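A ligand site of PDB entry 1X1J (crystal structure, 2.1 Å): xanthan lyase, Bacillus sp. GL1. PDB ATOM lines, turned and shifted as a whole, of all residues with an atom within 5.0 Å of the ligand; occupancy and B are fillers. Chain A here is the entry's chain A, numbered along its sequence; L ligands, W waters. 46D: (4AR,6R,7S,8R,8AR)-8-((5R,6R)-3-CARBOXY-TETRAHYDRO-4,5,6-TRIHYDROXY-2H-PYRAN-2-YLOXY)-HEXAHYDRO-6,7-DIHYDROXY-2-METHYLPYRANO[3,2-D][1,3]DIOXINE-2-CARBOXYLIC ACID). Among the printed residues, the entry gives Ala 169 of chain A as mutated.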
ATOM      1  N   ASN A  69       9.375   5.205  33.400  1.00  0.00           N
ATOM      2  CA  ASN A  69       8.166   4.704  34.044  1.00  0.00           C
ATOM      3  C   ASN A  69       8.527   3.584  35.021  1.00  0.00           C
ATOM      4  O   ASN A  69       7.961   3.495  36.114  1.00  0.00           O
ATOM      5  CB  ASN A  69       7.166   4.182  33.007  1.00  0.00           C
ATOM      6  CG  ASN A  69       5.807   3.892  33.608  1.00  0.00           C
ATOM      7  OD1 ASN A  69       5.443   2.739  33.847  1.00  0.00           O
ATOM      8  ND2 ASN A  69       5.048   4.935  33.893  1.00  0.00           N
ATOM      9  N   GLU A  73       8.153   3.302  39.112  1.00  0.00           N
ATOM     10  CA  GLU A  73       7.470   2.169  39.705  1.00  0.00           C
ATOM     11  C   GLU A  73       8.300   1.627  40.865  1.00  0.00           C
ATOM     12  O   GLU A  73       7.794   1.446  41.969  1.00  0.00           O
ATOM     13  CB  GLU A  73       7.238   1.069  38.674  1.00  0.00           C
ATOM     14  CG  GLU A  73       6.294   1.449  37.558  1.00  0.00           C
ATOM     15  CD  GLU A  73       5.872   0.262  36.714  1.00  0.00           C
ATOM     16  OE1 GLU A  73       6.756  -0.402  36.115  1.00  0.00           O
ATOM     17  OE2 GLU A  73       4.651  -0.020  36.661  1.00  0.00           O
ATOM     18  N   ASN A 121       6.785   7.458  25.143  1.00  0.00           N
ATOM     19  CA  ASN A 121       5.376   7.150  24.962  1.00  0.00           C
ATOM     20  C   ASN A 121       4.584   8.134  25.817  1.00  0.00           C
ATOM     21  O   ASN A 121       4.744   8.176  27.040  1.00  0.00           O
ATOM     22  CB  ASN A 121       5.106   5.705  25.420  1.00  0.00           C
ATOM     23  CG  ASN A 121       3.675   5.249  25.169  1.00  0.00           C
ATOM     24  OD1 ASN A 121       3.328   4.095  25.449  1.00  0.00           O
ATOM     25  ND2 ASN A 121       2.841   6.131  24.651  1.00  0.00           N
ATOM     26  N   TRP A 122       3.760   8.946  25.179  1.00  0.00           N
ATOM     27  CA  TRP A 122       2.959   9.948  25.886  1.00  0.00           C
ATOM     28  C   TRP A 122       2.267   9.376  27.121  1.00  0.00           C
ATOM     29  O   TRP A 122       2.136  10.068  28.132  1.00  0.00           O
ATOM     30  CB  TRP A 122       1.895  10.529  24.946  1.00  0.00           C
ATOM     31  CG  TRP A 122       0.842   9.531  24.611  1.00  0.00           C
ATOM     32  CD1 TRP A 122       0.894   8.597  23.628  1.00  0.00           C
ATOM     33  CD2 TRP A 122      -0.373   9.312  25.317  1.00  0.00           C
ATOM     34  NE1 TRP A 122      -0.232   7.794  23.675  1.00  0.00           N
ATOM     35  CE2 TRP A 122      -1.021   8.214  24.711  1.00  0.00           C
ATOM     36  CE3 TRP A 122      -0.992   9.937  26.413  1.00  0.00           C
ATOM     37  CZ2 TRP A 122      -2.250   7.728  25.158  1.00  0.00           C
ATOM     38  CZ3 TRP A 122      -2.215   9.447  26.866  1.00  0.00           C
ATOM     39  CH2 TRP A 122      -2.829   8.359  26.233  1.00  0.00           C
ATOM     40  N   TRP A 123       1.826   8.120  27.038  1.00  0.00           N
ATOM     41  CA  TRP A 123       1.123   7.467  28.136  1.00  0.00           C
ATOM     42  C   TRP A 123       1.930   7.459  29.432  1.00  0.00           C
ATOM     43  O   TRP A 123       1.382   7.683  30.504  1.00  0.00           O
ATOM     44  CB  TRP A 123       0.763   6.023  27.786  1.00  0.00           C
ATOM     45  CG  TRP A 123      -0.225   5.439  28.768  1.00  0.00           C
ATOM     46  CD1 TRP A 123      -1.590   5.571  28.727  1.00  0.00           C
ATOM     47  CD2 TRP A 123       0.077   4.741  29.977  1.00  0.00           C
ATOM     48  NE1 TRP A 123      -2.150   4.995  29.845  1.00  0.00           N
ATOM     49  CE2 TRP A 123      -1.152   4.478  30.629  1.00  0.00           C
ATOM     50  CE3 TRP A 123       1.272   4.306  30.581  1.00  0.00           C
ATOM     51  CZ2 TRP A 123      -1.228   3.813  31.853  1.00  0.00           C
ATOM     52  CZ3 TRP A 123       1.195   3.641  31.806  1.00  0.00           C
ATOM     53  CH2 TRP A 123      -0.050   3.399  32.425  1.00  0.00           C
ATOM     54  N   HIS A 124       3.229   7.195  29.319  1.00  0.00           N
ATOM     55  CA  HIS A 124       4.112   7.166  30.484  1.00  0.00           C
ATOM     56  C   HIS A 124       4.282   8.551  31.080  1.00  0.00           C
ATOM     57  O   HIS A 124       4.189   8.737  32.299  1.00  0.00           O
ATOM     58  CB  HIS A 124       5.487   6.631  30.083  1.00  0.00           C
ATOM     59  CG  HIS A 124       5.491   5.170  29.740  1.00  0.00           C
ATOM     60  ND1 HIS A 124       6.383   4.614  28.860  1.00  0.00           N
ATOM     61  CD2 HIS A 124       4.702   4.153  30.167  1.00  0.00           C
ATOM     62  CE1 HIS A 124       6.156   3.321  28.756  1.00  0.00           C
ATOM     63  NE2 HIS A 124       5.130   3.011  29.544  1.00  0.00           N
ATOM     64  N   ALA A 169      -8.075   6.175  29.415  1.00  0.00           N
ATOM     65  CA  ALA A 169      -7.216   7.352  29.435  1.00  0.00           C
ATOM     66  C   ALA A 169      -7.826   8.454  30.292  1.00  0.00           C
ATOM     67  O   ALA A 169      -7.152   9.048  31.134  1.00  0.00           O
ATOM     68  CB  ALA A 169      -6.994   7.862  28.002  1.00  0.00           C
ATOM     69  N   TRP A 172      -7.683   7.569  33.922  1.00  0.00           N
ATOM     70  CA  TRP A 172      -6.321   7.696  34.413  1.00  0.00           C
ATOM     71  C   TRP A 172      -5.989   9.163  34.638  1.00  0.00           C
ATOM     72  O   TRP A 172      -5.324   9.508  35.613  1.00  0.00           O
ATOM     73  CB  TRP A 172      -5.333   7.052  33.438  1.00  0.00           C
ATOM     74  CG  TRP A 172      -5.238   5.562  33.589  1.00  0.00           C
ATOM     75  CD1 TRP A 172      -5.175   4.852  34.758  1.00  0.00           C
ATOM     76  CD2 TRP A 172      -5.097   4.596  32.531  1.00  0.00           C
ATOM     77  NE1 TRP A 172      -4.991   3.512  34.495  1.00  0.00           N
ATOM     78  CE2 TRP A 172      -4.944   3.325  33.142  1.00  0.00           C
ATOM     79  CE3 TRP A 172      -5.075   4.676  31.132  1.00  0.00           C
ATOM     80  CZ2 TRP A 172      -4.778   2.145  32.398  1.00  0.00           C
ATOM     81  CZ3 TRP A 172      -4.905   3.505  30.388  1.00  0.00           C
ATOM     82  CH2 TRP A 172      -4.757   2.256  31.030  1.00  0.00           C
ATOM     83  N   HIS A 221     -10.555   1.912  21.961  1.00  0.00           N
ATOM     84  CA  HIS A 221      -9.858   2.143  20.710  1.00  0.00           C
ATOM     85  C   HIS A 221     -10.776   1.884  19.504  1.00  0.00           C
ATOM     86  O   HIS A 221     -10.352   1.350  18.483  1.00  0.00           O
ATOM     87  CB  HIS A 221      -8.606   1.253  20.603  1.00  0.00           C
ATOM     88  CG  HIS A 221      -7.496   1.672  21.508  1.00  0.00           C
ATOM     89  ND1 HIS A 221      -6.244   1.093  21.474  1.00  0.00           N
ATOM     90  CD2 HIS A 221      -7.447   2.606  22.483  1.00  0.00           C
ATOM     91  CE1 HIS A 221      -5.468   1.648  22.389  1.00  0.00           C
ATOM     92  NE2 HIS A 221      -6.182   2.574  23.017  1.00  0.00           N
ATOM     93  N   TYR A 230      -8.460  -2.815  28.915  1.00  0.00           N
ATOM     94  CA  TYR A 230      -8.709  -1.421  29.254  1.00  0.00           C
ATOM     95  C   TYR A 230      -9.923  -1.310  30.190  1.00  0.00           C
ATOM     96  O   TYR A 230     -10.008  -0.379  30.995  1.00  0.00           O
ATOM     97  CB  TYR A 230      -8.934  -0.608  27.984  1.00  0.00           C
ATOM     98  CG  TYR A 230      -7.652  -0.200  27.280  1.00  0.00           C
ATOM     99  CD1 TYR A 230      -6.814   0.777  27.815  1.00  0.00           C
ATOM    100  CD2 TYR A 230      -7.305  -0.759  26.052  1.00  0.00           C
ATOM    101  CE1 TYR A 230      -5.657   1.194  27.150  1.00  0.00           C
ATOM    102  CE2 TYR A 230      -6.150  -0.363  25.378  1.00  0.00           C
ATOM    103  CZ  TYR A 230      -5.335   0.611  25.934  1.00  0.00           C
ATOM    104  OH  TYR A 230      -4.202   1.029  25.248  1.00  0.00           O
ATOM    105  N   SER A 233      -8.926  -1.617  33.713  1.00  0.00           N
ATOM    106  CA  SER A 233      -8.295  -0.374  34.126  1.00  0.00           C
ATOM    107  C   SER A 233      -9.340   0.676  34.501  1.00  0.00           C
ATOM    108  O   SER A 233      -9.231   1.314  35.546  1.00  0.00           O
ATOM    109  CB  SER A 233      -7.397   0.163  33.000  1.00  0.00           C
ATOM    110  OG  SER A 233      -6.319  -0.738  32.760  1.00  0.00           O
ATOM    111  N   ARG A 284      -4.627  -6.783  23.260  1.00  0.00           N
ATOM    112  CA  ARG A 284      -3.210  -7.078  23.151  1.00  0.00           C
ATOM    113  C   ARG A 284      -2.552  -7.417  24.481  1.00  0.00           C
ATOM    114  O   ARG A 284      -1.397  -7.817  24.514  1.00  0.00           O
ATOM    115  CB  ARG A 284      -2.468  -5.909  22.476  1.00  0.00           C
ATOM    116  CG  ARG A 284      -2.309  -4.650  23.315  1.00  0.00           C
ATOM    117  CD  ARG A 284      -1.508  -3.597  22.537  1.00  0.00           C
ATOM    118  NE  ARG A 284      -0.960  -2.565  23.400  1.00  0.00           N
ATOM    119  CZ  ARG A 284      -1.685  -1.645  24.035  1.00  0.00           C
ATOM    120  NH1 ARG A 284      -3.005  -1.613  23.899  1.00  0.00           N
ATOM    121  NH2 ARG A 284      -1.076  -0.767  24.833  1.00  0.00           N
ATOM    122  N   GLU A 285      -3.294  -7.285  25.561  1.00  0.00           N
ATOM    123  CA  GLU A 285      -2.734  -7.580  26.876  1.00  0.00           C
ATOM    124  C   GLU A 285      -2.502  -9.081  27.095  1.00  0.00           C
ATOM    125  O   GLU A 285      -1.832  -9.470  28.059  1.00  0.00           O
ATOM    126  CB  GLU A 285      -3.642  -7.016  27.984  1.00  0.00           C
ATOM    127  CG  GLU A 285      -3.636  -5.477  28.028  1.00  0.00           C
ATOM    128  CD  GLU A 285      -4.405  -4.926  29.219  1.00  0.00           C
ATOM    129  OE1 GLU A 285      -4.359  -5.556  30.296  1.00  0.00           O
ATOM    130  OE2 GLU A 285      -5.040  -3.848  29.087  1.00  0.00           O
ATOM    131  N   ARG A 288       1.013 -10.069  27.525  1.00  0.00           N
ATOM    132  CA  ARG A 288       1.725  -9.553  28.708  1.00  0.00           C
ATOM    133  C   ARG A 288       1.880 -10.624  29.777  1.00  0.00           C
ATOM    134  O   ARG A 288       0.891 -11.074  30.366  1.00  0.00           O
ATOM    135  CB  ARG A 288       0.993  -8.340  29.278  1.00  0.00           C
ATOM    136  CG  ARG A 288       1.026  -7.135  28.360  1.00  0.00           C
ATOM    137  CD  ARG A 288       0.221  -5.965  28.920  1.00  0.00           C
ATOM    138  NE  ARG A 288       0.253  -4.836  27.995  1.00  0.00           N
ATOM    139  CZ  ARG A 288      -0.349  -3.671  28.218  1.00  0.00           C
ATOM    140  NH1 ARG A 288      -1.032  -3.480  29.331  1.00  0.00           N
ATOM    141  NH2 ARG A 288      -0.250  -2.694  27.328  1.00  0.00           N
ATOM    142  N   TYR A 290       2.941 -10.457  32.812  1.00  0.00           N
ATOM    143  CA  TYR A 290       2.463 -10.068  34.140  1.00  0.00           C
ATOM    144  C   TYR A 290       0.949  -9.903  34.218  1.00  0.00           C
ATOM    145  O   TYR A 290       0.415  -9.576  35.285  1.00  0.00           O
ATOM    146  CB  TYR A 290       3.122  -8.763  34.573  1.00  0.00           C
ATOM    147  CG  TYR A 290       3.052  -7.676  33.531  1.00  0.00           C
ATOM    148  CD1 TYR A 290       4.026  -7.568  32.542  1.00  0.00           C
ATOM    149  CD2 TYR A 290       1.996  -6.763  33.517  1.00  0.00           C
ATOM    150  CE1 TYR A 290       3.953  -6.585  31.569  1.00  0.00           C
ATOM    151  CE2 TYR A 290       1.914  -5.766  32.546  1.00  0.00           C
ATOM    152  CZ  TYR A 290       2.896  -5.695  31.573  1.00  0.00           C
ATOM    153  OH  TYR A 290       2.842  -4.721  30.607  1.00  0.00           O
ATOM    154  N   ILE A 398      -0.148  -3.107  18.886  1.00  0.00           N
ATOM    155  CA  ILE A 398       0.577  -1.852  18.809  1.00  0.00           C
ATOM    156  C   ILE A 398       1.730  -1.950  19.793  1.00  0.00           C
ATOM    157  O   ILE A 398       1.754  -2.836  20.655  1.00  0.00           O
ATOM    158  CB  ILE A 398      -0.315  -0.625  19.155  1.00  0.00           C
ATOM    159  CG1 ILE A 398      -0.849  -0.734  20.579  1.00  0.00           C
ATOM    160  CG2 ILE A 398      -1.461  -0.527  18.149  1.00  0.00           C
ATOM    161  CD1 ILE A 398      -1.643   0.495  21.024  1.00  0.00           C
ATOM    162  N   ASN A 399       2.687  -1.044  19.666  1.00  0.00           N
ATOM    163  CA  ASN A 399       3.866  -1.013  20.527  1.00  0.00           C
ATOM    164  C   ASN A 399       4.564  -2.367  20.619  1.00  0.00           C
ATOM    165  O   ASN A 399       5.093  -2.734  21.657  1.00  0.00           O
ATOM    166  CB  ASN A 399       3.497  -0.523  21.920  1.00  0.00           C
ATOM    167  CG  ASN A 399       2.844   0.838  21.906  1.00  0.00           C
ATOM    168  OD1 ASN A 399       3.256   1.720  21.152  1.00  0.00           O
ATOM    169  ND2 ASN A 399       1.834   1.020  22.753  1.00  0.00           N
ATOM    170  N   ARG A 587       9.111  -5.667  23.888  1.00  0.00           N
ATOM    171  CA  ARG A 587       9.389  -4.440  24.624  1.00  0.00           C
ATOM    172  C   ARG A 587      10.599  -4.731  25.511  1.00  0.00           C
ATOM    173  O   ARG A 587      10.733  -5.822  26.040  1.00  0.00           O
ATOM    174  CB  ARG A 587       8.193  -4.011  25.468  1.00  0.00           C
ATOM    175  CG  ARG A 587       6.998  -3.567  24.630  1.00  0.00           C
ATOM    176  CD  ARG A 587       5.874  -3.064  25.516  1.00  0.00           C
ATOM    177  NE  ARG A 587       5.488  -4.075  26.492  1.00  0.00           N
ATOM    178  CZ  ARG A 587       4.702  -3.844  27.532  1.00  0.00           C
ATOM    179  NH1 ARG A 587       4.212  -2.617  27.738  1.00  0.00           N
ATOM    180  NH2 ARG A 587       4.405  -4.828  28.375  1.00  0.00           N
HETATM  181  O6A 46D L   1      -5.135   3.967  25.385  1.00  0.00           O
HETATM  182  C6  46D L   1      -3.985   3.978  25.875  1.00  0.00           C
HETATM  183  O6B 46D L   1      -3.743   4.227  27.081  1.00  0.00           O
HETATM  184  C5  46D L   1      -2.809   3.709  24.940  1.00  0.00           C
HETATM  185  O5  46D L   1      -2.451   4.935  24.282  1.00  0.00           O
HETATM  186  C1  46D L   1      -1.410   4.750  23.314  1.00  0.00           C
HETATM  187  C2  46D L   1      -0.137   4.271  24.027  1.00  0.00           C
HETATM  188  O2  46D L   1       0.891   4.036  23.061  1.00  0.00           O
HETATM  189  C3  46D L   1      -0.427   2.973  24.790  1.00  0.00           C
HETATM  190  O3  46D L   1       0.727   2.640  25.561  1.00  0.00           O
HETATM  191  C4  46D L   1      -1.628   3.133  25.723  1.00  0.00           C
HETATM  192  OP1 46D L   1      -2.011   1.862  26.277  1.00  0.00           O
HETATM  193  CP1 46D L   1      -1.557   1.708  27.634  1.00  0.00           C
HETATM  194  OP5 46D L   1      -0.144   1.457  27.671  1.00  0.00           O
HETATM  195  CP5 46D L   1       0.343   1.345  29.018  1.00  0.00           C
HETATM  196  CP6 46D L   1       1.845   1.122  29.041  1.00  0.00           C
HETATM  197  OP6 46D L   1       2.287   0.995  30.408  1.00  0.00           O
HETATM  198  CP7 46D L   1       1.641  -0.067  31.135  1.00  0.00           C
HETATM  199  CP9 46D L   1       2.106  -1.445  30.652  1.00  0.00           C
HETATM  200  OP7 46D L   1       1.330  -2.403  30.843  1.00  0.00           O
HETATM  201  OP8 46D L   1       3.230  -1.506  30.099  1.00  0.00           O
HETATM  202  CP8 46D L   1       2.038   0.080  32.599  1.00  0.00           C
HETATM  203  OP4 46D L   1       0.214   0.051  31.058  1.00  0.00           O
HETATM  204  CP4 46D L   1      -0.278   0.133  29.701  1.00  0.00           C
HETATM  205  CP3 46D L   1      -1.789   0.314  29.709  1.00  0.00           C
HETATM  206  OP3 46D L   1      -2.406  -0.854  30.248  1.00  0.00           O
HETATM  207  CP2 46D L   1      -2.312   0.547  28.282  1.00  0.00           C
HETATM  208  OP2 46D L   1      -2.090  -0.644  27.521  1.00  0.00           O
HETATM  209  O   HOH W   1       1.819  -0.577  25.183  1.00  0.00           O
HETATM  210  O   HOH W   2      -4.180   5.883  22.497  1.00  0.00           O
HETATM  211  O   HOH W   3      -2.468   7.077  21.165  1.00  0.00           O
HETATM  212  O   HOH W   4      -7.918   4.843  26.703  1.00  0.00           O
HETATM  213  O   HOH W   5      -4.039  -2.469  26.965  1.00  0.00           O
HETATM  214  O   HOH W   6       4.792   0.175  29.347  1.00  0.00           O
HETATM  215  O   HOH W   7      -5.071  -1.368  30.327  1.00  0.00           O
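The side-chain hydroxyl (OH) of Tyr 230 lies within hydrogen-bond range of an oxygen (OP1) of the ligand (2.6 Å).
OP7 of the ligand lies within salt-bridge range of NH1 of Arg 288.
OP7 of the ligand sits at hydrogen-bond distance from OH of Tyr 290.
An oxygen (OP8) of the ligand is in salt-bridge range of the guanidinium group (NH1) of Arg 587 (2.8 Å).
The guanidinium group (NH2) of Arg 284 sits at hydrogen-bond distance from an oxygen (OP2) of the ligand, at 2.9 Å.
A ring nitrogen (NE2) of His 221 lies within hydrogen-bond range of an oxygen (O6A) of the ligand, at 2.9 Å.
An oxygen (O3) of the ligand lies within hydrogen-bond range of the side-chain amide oxygen (OD1) of Asn 121 (3.0 Å).
An oxygen (O6B) of the ligand lies close to the indole nitrogen (NE1) of Trp 123 (3.3 Å).
O2 of the ligand lies within hydrogen-bond range of ND2 of Asn 399 (3.2 Å).
The side-chain hydroxyl (OH) of Tyr 230 sits at hydrogen-bond distance from the guanidinium group (NH1) of Arg 284, at 3.2 Å.
NE2 of His 221 sits close to OH of Tyr 230, 3.4 Å away.
OH of Tyr 290 is in hydrogen-bond range of NH2 of Arg 587, at 2.7 Å.
The backbone NH of Trp 123 sits close to the side-chain amide nitrogen of Asn 121.
Trp 122 touches the ligand.
NE2 of His 124 touches OP6 of the ligand (3.6 Å).
Trp 172 touches the ligand.
12 residues have an atom within 4 Å of the ligand: Asn 121, Trp 122, Trp 123, His 124, Trp 172, His 221, Tyr 230, Arg 284, Arg 288, Tyr 290, Asn 399 and Arg 587.
The nearest printed residue that does not touch the ligand is Glu 285 (4.2 Å).
Water W6 lies within hydrogen-bond range of OP8 of the ligand (2.4 Å), NE2 of His 124 (2.9 Å) and NH1 of Arg 587 (3.3 Å).
Water W7 lies within hydrogen-bond range of OP3 of the ligand, OE2 of Glu 285 and OG of Ser 233.
Water W5 lies within hydrogen-bond range of OE2 of Glu 285 (2.7 Å), OP2 of the ligand (2.7 Å) and NH1 of Arg 284 (3.3 Å).
Water W4 lies within hydrogen-bond range of N of Ala 169 (3.0 Å) and O6A of the ligand (3.2 Å).
Water W1 lies within hydrogen-bond range of ND2 of Asn 399 (2.9 Å), NH2 of Arg 284 (2.9 Å) and O3 of the ligand (3.4 Å).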
